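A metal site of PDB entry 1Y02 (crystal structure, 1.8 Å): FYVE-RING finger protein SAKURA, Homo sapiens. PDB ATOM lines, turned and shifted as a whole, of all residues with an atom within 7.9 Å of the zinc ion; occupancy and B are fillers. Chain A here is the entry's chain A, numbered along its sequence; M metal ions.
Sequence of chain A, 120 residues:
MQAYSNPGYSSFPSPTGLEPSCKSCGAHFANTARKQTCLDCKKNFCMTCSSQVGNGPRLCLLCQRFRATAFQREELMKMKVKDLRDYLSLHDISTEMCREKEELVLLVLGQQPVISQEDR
SG of Cys 63 sits close to NE2 of His 91, 3.4 Å away.
The side-chain sulfur (SG) of Cys 38 lies close to the backbone NH (N) of Asp 40 (3.5 Å).
The backbone carbonyl oxygen (O) of Lys 43 lies within hydrogen-bond range of the backbone NH (N) of Cys 38 (3.0 Å).
SG of Cys 41 sits close to N of Lys 43, at 3.6 Å.
The zinc ion is bound by the side-chain sulfur of Cys 41 (2.4 Å), the side-chain sulfur of Cys 63 (2.4 Å), the side-chain sulfur of Cys 60 (2.4 Å) and the side-chain sulfur of Cys 38 (2.4 Å).
Four residues have an atom within 4 Å of the zinc ion: Cys 38, Cys 41, Cys 60 and Cys 63.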
ATOM      1  N   LYS A  23      25.222  16.833  11.723  1.00  0.00           N
ATOM      2  CA  LYS A  23      24.524  17.982  12.281  1.00  0.00           C
ATOM      3  C   LYS A  23      23.233  17.592  13.011  1.00  0.00           C
ATOM      4  O   LYS A  23      22.789  18.298  13.905  1.00  0.00           O
ATOM      5  CB  LYS A  23      24.223  18.972  11.146  1.00  0.00           C
ATOM      6  CG  LYS A  23      23.503  20.251  11.574  1.00  0.00           C
ATOM      7  CD  LYS A  23      24.332  21.104  12.531  1.00  0.00           C
ATOM      8  CE  LYS A  23      25.568  21.666  11.862  1.00  0.00           C
ATOM      9  NZ  LYS A  23      26.388  22.465  12.833  1.00  0.00           N
ATOM     10  N   THR A  37      26.424  15.825   2.404  1.00  0.00           N
ATOM     11  CA  THR A  37      26.205  17.261   2.526  1.00  0.00           C
ATOM     12  C   THR A  37      24.844  17.604   1.957  1.00  0.00           C
ATOM     13  O   THR A  37      24.533  17.256   0.823  1.00  0.00           O
ATOM     14  CB  THR A  37      27.277  18.059   1.758  1.00  0.00           C
ATOM     15  OG1 THR A  37      28.588  17.705   2.237  1.00  0.00           O
ATOM     16  CG2 THR A  37      27.067  19.556   1.944  1.00  0.00           C
ATOM     17  N   CYS A  38      24.013  18.289   2.746  1.00  0.00           N
ATOM     18  CA  CYS A  38      22.677  18.667   2.305  1.00  0.00           C
ATOM     19  C   CYS A  38      22.785  19.809   1.298  1.00  0.00           C
ATOM     20  O   CYS A  38      23.397  20.826   1.580  1.00  0.00           O
ATOM     21  CB  CYS A  38      21.830  19.103   3.501  1.00  0.00           C
ATOM     22  SG  CYS A  38      20.154  19.618   3.056  1.00  0.00           S
ATOM     23  N   LEU A  39      22.168  19.628   0.138  1.00  0.00           N
ATOM     24  CA  LEU A  39      22.213  20.656  -0.902  1.00  0.00           C
ATOM     25  C   LEU A  39      21.533  21.961  -0.490  1.00  0.00           C
ATOM     26  O   LEU A  39      21.859  23.035  -1.011  1.00  0.00           O
ATOM     27  CB  LEU A  39      21.556  20.122  -2.184  1.00  0.00           C
ATOM     28  CG  LEU A  39      21.693  21.005  -3.435  1.00  0.00           C
ATOM     29  CD1 LEU A  39      23.164  21.104  -3.819  1.00  0.00           C
ATOM     30  CD2 LEU A  39      20.896  20.390  -4.576  1.00  0.00           C
ATOM     31  N   ASP A  40      20.611  21.868   0.462  1.00  0.00           N
ATOM     32  CA  ASP A  40      19.880  23.047   0.931  1.00  0.00           C
ATOM     33  C   ASP A  40      20.543  23.820   2.074  1.00  0.00           C
ATOM     34  O   ASP A  40      20.813  25.010   1.927  1.00  0.00           O
ATOM     35  CB  ASP A  40      18.463  22.664   1.340  1.00  0.00           C
ATOM     36  CG  ASP A  40      17.521  22.595   0.149  1.00  0.00           C
ATOM     37  OD1 ASP A  40      16.298  22.474   0.367  1.00  0.00           O
ATOM     38  OD2 ASP A  40      18.006  22.657  -0.997  1.00  0.00           O
ATOM     39  N   CYS A  41      20.784  23.160   3.211  1.00  0.00           N
ATOM     40  CA  CYS A  41      21.414  23.865   4.325  1.00  0.00           C
ATOM     41  C   CYS A  41      22.938  23.764   4.282  1.00  0.00           C
ATOM     42  O   CYS A  41      23.633  24.505   4.976  1.00  0.00           O
ATOM     43  CB  CYS A  41      20.889  23.329   5.675  1.00  0.00           C
ATOM     44  SG  CYS A  41      21.302  21.613   6.045  1.00  0.00           S
ATOM     45  N   LYS A  42      23.443  22.856   3.459  1.00  0.00           N
ATOM     46  CA  LYS A  42      24.869  22.650   3.271  1.00  0.00           C
ATOM     47  C   LYS A  42      25.618  22.096   4.470  1.00  0.00           C
ATOM     48  O   LYS A  42      26.845  22.137   4.517  1.00  0.00           O
ATOM     49  CB  LYS A  42      25.537  23.952   2.800  1.00  0.00           C
ATOM     50  CG  LYS A  42      24.888  24.514   1.531  1.00  0.00           C
ATOM     51  CD  LYS A  42      25.731  25.593   0.893  1.00  0.00           C
ATOM     52  CE  LYS A  42      25.032  26.161  -0.336  1.00  0.00           C
ATOM     53  NZ  LYS A  42      24.593  25.077  -1.279  1.00  0.00           N
ATOM     54  N   LYS A  43      24.893  21.571   5.456  1.00  0.00           N
ATOM     55  CA  LYS A  43      25.529  20.987   6.621  1.00  0.00           C
ATOM     56  C   LYS A  43      25.784  19.502   6.332  1.00  0.00           C
ATOM     57  O   LYS A  43      25.251  18.958   5.358  1.00  0.00           O
ATOM     58  CB  LYS A  43      24.653  21.163   7.864  1.00  0.00           C
ATOM     59  CG  LYS A  43      24.244  22.611   8.147  1.00  0.00           C
ATOM     60  CD  LYS A  43      25.430  23.566   8.113  1.00  0.00           C
ATOM     61  CE  LYS A  43      24.977  25.010   8.333  1.00  0.00           C
ATOM     62  NZ  LYS A  43      26.104  25.997   8.223  1.00  0.00           N
ATOM     63  N   ASN A  44      26.601  18.837   7.160  1.00  0.00           N
ATOM     64  CA  ASN A  44      26.912  17.424   6.952  1.00  0.00           C
ATOM     65  C   ASN A  44      26.034  16.491   7.788  1.00  0.00           C
ATOM     66  O   ASN A  44      25.747  16.786   8.936  1.00  0.00           O
ATOM     67  CB  ASN A  44      28.396  17.157   7.272  1.00  0.00           C
ATOM     68  CG  ASN A  44      29.330  18.023   6.454  1.00  0.00           C
ATOM     69  OD1 ASN A  44      29.160  18.176   5.249  1.00  0.00           O
ATOM     70  ND2 ASN A  44      30.330  18.599   7.114  1.00  0.00           N
ATOM     71  N   PHE A  45      25.627  15.366   7.191  1.00  0.00           N
ATOM     72  CA  PHE A  45      24.742  14.410   7.869  1.00  0.00           C
ATOM     73  C   PHE A  45      25.052  12.956   7.567  1.00  0.00           C
ATOM     74  O   PHE A  45      25.736  12.636   6.599  1.00  0.00           O
ATOM     75  CB  PHE A  45      23.294  14.626   7.441  1.00  0.00           C
ATOM     76  CG  PHE A  45      22.791  16.012   7.657  1.00  0.00           C
ATOM     77  CD1 PHE A  45      23.056  17.019   6.742  1.00  0.00           C
ATOM     78  CD2 PHE A  45      22.024  16.305   8.779  1.00  0.00           C
ATOM     79  CE1 PHE A  45      22.573  18.310   6.938  1.00  0.00           C
ATOM     80  CE2 PHE A  45      21.538  17.593   8.991  1.00  0.00           C
ATOM     81  CZ  PHE A  45      21.819  18.597   8.073  1.00  0.00           C
ATOM     82  N   CYS A  49      20.539  10.063   8.151  1.00  0.00           N
ATOM     83  CA  CYS A  49      19.952  11.334   8.571  1.00  0.00           C
ATOM     84  C   CYS A  49      19.695  12.226   7.361  1.00  0.00           C
ATOM     85  O   CYS A  49      19.584  13.442   7.478  1.00  0.00           O
ATOM     86  CB  CYS A  49      20.868  12.048   9.570  1.00  0.00           C
ATOM     87  SG  CYS A  49      20.953  11.234  11.184  1.00  0.00           S
ATOM     88  N   SER A  50      19.627  11.598   6.190  1.00  0.00           N
ATOM     89  CA  SER A  50      19.368  12.307   4.941  1.00  0.00           C
ATOM     90  C   SER A  50      18.585  11.376   4.022  1.00  0.00           C
ATOM     91  O   SER A  50      18.411  10.205   4.335  1.00  0.00           O
ATOM     92  CB  SER A  50      20.687  12.738   4.291  1.00  0.00           C
ATOM     93  OG  SER A  50      21.560  11.648   4.080  1.00  0.00           O
ATOM     94  N   ARG A  58      20.564  15.262  -2.752  1.00  0.00           N
ATOM     95  CA  ARG A  58      20.747  14.732  -1.401  1.00  0.00           C
ATOM     96  C   ARG A  58      20.360  15.824  -0.404  1.00  0.00           C
ATOM     97  O   ARG A  58      20.960  16.902  -0.386  1.00  0.00           O
ATOM     98  CB  ARG A  58      22.207  14.323  -1.198  1.00  0.00           C
ATOM     99  CG  ARG A  58      22.578  13.975   0.237  1.00  0.00           C
ATOM    100  CD  ARG A  58      21.708  12.856   0.794  1.00  0.00           C
ATOM    101  NE  ARG A  58      21.750  11.641  -0.016  1.00  0.00           N
ATOM    102  CZ  ARG A  58      21.317  10.460   0.399  1.00  0.00           C
ATOM    103  NH1 ARG A  58      21.385   9.404  -0.411  1.00  0.00           N
ATOM    104  NH2 ARG A  58      20.814  10.321   1.620  1.00  0.00           N
ATOM    105  N   LEU A  59      19.360  15.538   0.434  1.00  0.00           N
ATOM    106  CA  LEU A  59      18.883  16.493   1.418  1.00  0.00           C
ATOM    107  C   LEU A  59      18.785  15.876   2.813  1.00  0.00           C
ATOM    108  O   LEU A  59      18.599  14.666   2.952  1.00  0.00           O
ATOM    109  CB  LEU A  59      17.497  17.017   1.021  1.00  0.00           C
ATOM    110  CG  LEU A  59      17.334  17.689  -0.346  1.00  0.00           C
ATOM    111  CD1 LEU A  59      15.863  17.958  -0.603  1.00  0.00           C
ATOM    112  CD2 LEU A  59      18.132  18.985  -0.391  1.00  0.00           C
ATOM    113  N   CYS A  60      18.926  16.689   3.854  1.00  0.00           N
ATOM    114  CA  CYS A  60      18.792  16.151   5.201  1.00  0.00           C
ATOM    115  C   CYS A  60      17.283  15.951   5.379  1.00  0.00           C
ATOM    116  O   CYS A  60      16.497  16.467   4.586  1.00  0.00           O
ATOM    117  CB  CYS A  60      19.372  17.091   6.249  1.00  0.00           C
ATOM    118  SG  CYS A  60      18.494  18.638   6.509  1.00  0.00           S
ATOM    119  N   LEU A  61      16.888  15.200   6.399  1.00  0.00           N
ATOM    120  CA  LEU A  61      15.472  14.922   6.611  1.00  0.00           C
ATOM    121  C   LEU A  61      14.583  16.144   6.839  1.00  0.00           C
ATOM    122  O   LEU A  61      13.430  16.160   6.402  1.00  0.00           O
ATOM    123  CB  LEU A  61      15.312  13.930   7.759  1.00  0.00           C
ATOM    124  CG  LEU A  61      16.057  12.607   7.530  1.00  0.00           C
ATOM    125  CD1 LEU A  61      15.757  11.649   8.673  1.00  0.00           C
ATOM    126  CD2 LEU A  61      15.643  11.997   6.199  1.00  0.00           C
ATOM    127  N   LEU A  62      15.105  17.172   7.499  1.00  0.00           N
ATOM    128  CA  LEU A  62      14.305  18.366   7.742  1.00  0.00           C
ATOM    129  C   LEU A  62      14.151  19.197   6.469  1.00  0.00           C
ATOM    130  O   LEU A  62      13.043  19.637   6.137  1.00  0.00           O
ATOM    131  CB  LEU A  62      14.946  19.202   8.859  1.00  0.00           C
ATOM    132  CG  LEU A  62      14.035  20.209   9.562  1.00  0.00           C
ATOM    133  CD1 LEU A  62      12.816  19.496  10.143  1.00  0.00           C
ATOM    134  CD2 LEU A  62      14.812  20.921  10.662  1.00  0.00           C
ATOM    135  N   CYS A  63      15.235  19.402   5.734  1.00  0.00           N
ATOM    136  CA  CYS A  63      15.145  20.186   4.509  1.00  0.00           C
ATOM    137  C   CYS A  63      14.270  19.455   3.490  1.00  0.00           C
ATOM    138  O   CYS A  63      13.582  20.095   2.697  1.00  0.00           O
ATOM    139  CB  CYS A  63      16.534  20.435   3.931  1.00  0.00           C
ATOM    140  SG  CYS A  63      17.464  21.664   4.863  1.00  0.00           S
ATOM    141  N   GLN A  64      14.282  18.131   3.534  1.00  0.00           N
ATOM    142  CA  GLN A  64      13.456  17.334   2.616  1.00  0.00           C
ATOM    143  C   GLN A  64      11.999  17.563   2.985  1.00  0.00           C
ATOM    144  O   GLN A  64      11.144  17.756   2.114  1.00  0.00           O
ATOM    145  CB  GLN A  64      13.794  15.852   2.776  1.00  0.00           C
ATOM    146  CG  GLN A  64      13.096  14.925   1.783  1.00  0.00           C
ATOM    147  CD  GLN A  64      13.653  15.047   0.374  1.00  0.00           C
ATOM    148  OE1 GLN A  64      13.278  15.948  -0.385  1.00  0.00           O
ATOM    149  NE2 GLN A  64      14.568  14.150   0.025  1.00  0.00           N
ATOM    150  N   TYR A  87      14.932  24.123  11.445  1.00  0.00           N
ATOM    151  CA  TYR A  87      15.156  24.325  10.014  1.00  0.00           C
ATOM    152  C   TYR A  87      15.857  25.657   9.798  1.00  0.00           C
ATOM    153  O   TYR A  87      16.844  25.752   9.068  1.00  0.00           O
ATOM    154  CB  TYR A  87      13.823  24.297   9.258  1.00  0.00           C
ATOM    155  CG  TYR A  87      13.933  24.577   7.784  1.00  0.00           C
ATOM    156  CD1 TYR A  87      14.354  23.584   6.890  1.00  0.00           C
ATOM    157  CD2 TYR A  87      13.606  25.825   7.274  1.00  0.00           C
ATOM    158  CE1 TYR A  87      14.447  23.840   5.516  1.00  0.00           C
ATOM    159  CE2 TYR A  87      13.685  26.096   5.907  1.00  0.00           C
ATOM    160  CZ  TYR A  87      14.109  25.097   5.036  1.00  0.00           C
ATOM    161  OH  TYR A  87      14.151  25.368   3.692  1.00  0.00           O
ATOM    162  N   LEU A  90      19.486  25.521  10.856  1.00  0.00           N
ATOM    163  CA  LEU A  90      20.326  24.821   9.896  1.00  0.00           C
ATOM    164  C   LEU A  90      20.732  25.749   8.764  1.00  0.00           C
ATOM    165  O   LEU A  90      21.792  25.589   8.160  1.00  0.00           O
ATOM    166  CB  LEU A  90      19.591  23.619   9.306  1.00  0.00           C
ATOM    167  CG  LEU A  90      19.417  22.415  10.232  1.00  0.00           C
ATOM    168  CD1 LEU A  90      18.608  21.329   9.512  1.00  0.00           C
ATOM    169  CD2 LEU A  90      20.789  21.888  10.626  1.00  0.00           C
ATOM    170  N   HIS A  91      19.874  26.714   8.471  1.00  0.00           N
ATOM    171  CA  HIS A  91      20.127  27.681   7.411  1.00  0.00           C
ATOM    172  C   HIS A  91      20.795  28.945   7.950  1.00  0.00           C
ATOM    173  O   HIS A  91      20.877  29.959   7.263  1.00  0.00           O
ATOM    174  CB  HIS A  91      18.804  27.996   6.698  1.00  0.00           C
ATOM    175  CG  HIS A  91      18.315  26.873   5.851  1.00  0.00           C
ATOM    176  ND1 HIS A  91      18.597  26.773   4.509  1.00  0.00           N
ATOM    177  CD2 HIS A  91      17.613  25.753   6.167  1.00  0.00           C
ATOM    178  CE1 HIS A  91      18.090  25.648   4.032  1.00  0.00           C
ATOM    179  NE2 HIS A  91      17.493  25.011   5.014  1.00  0.00           N
HETATM  180 ZN    ZN M   1      19.441  20.421   5.215  1.00  0.00          ZN
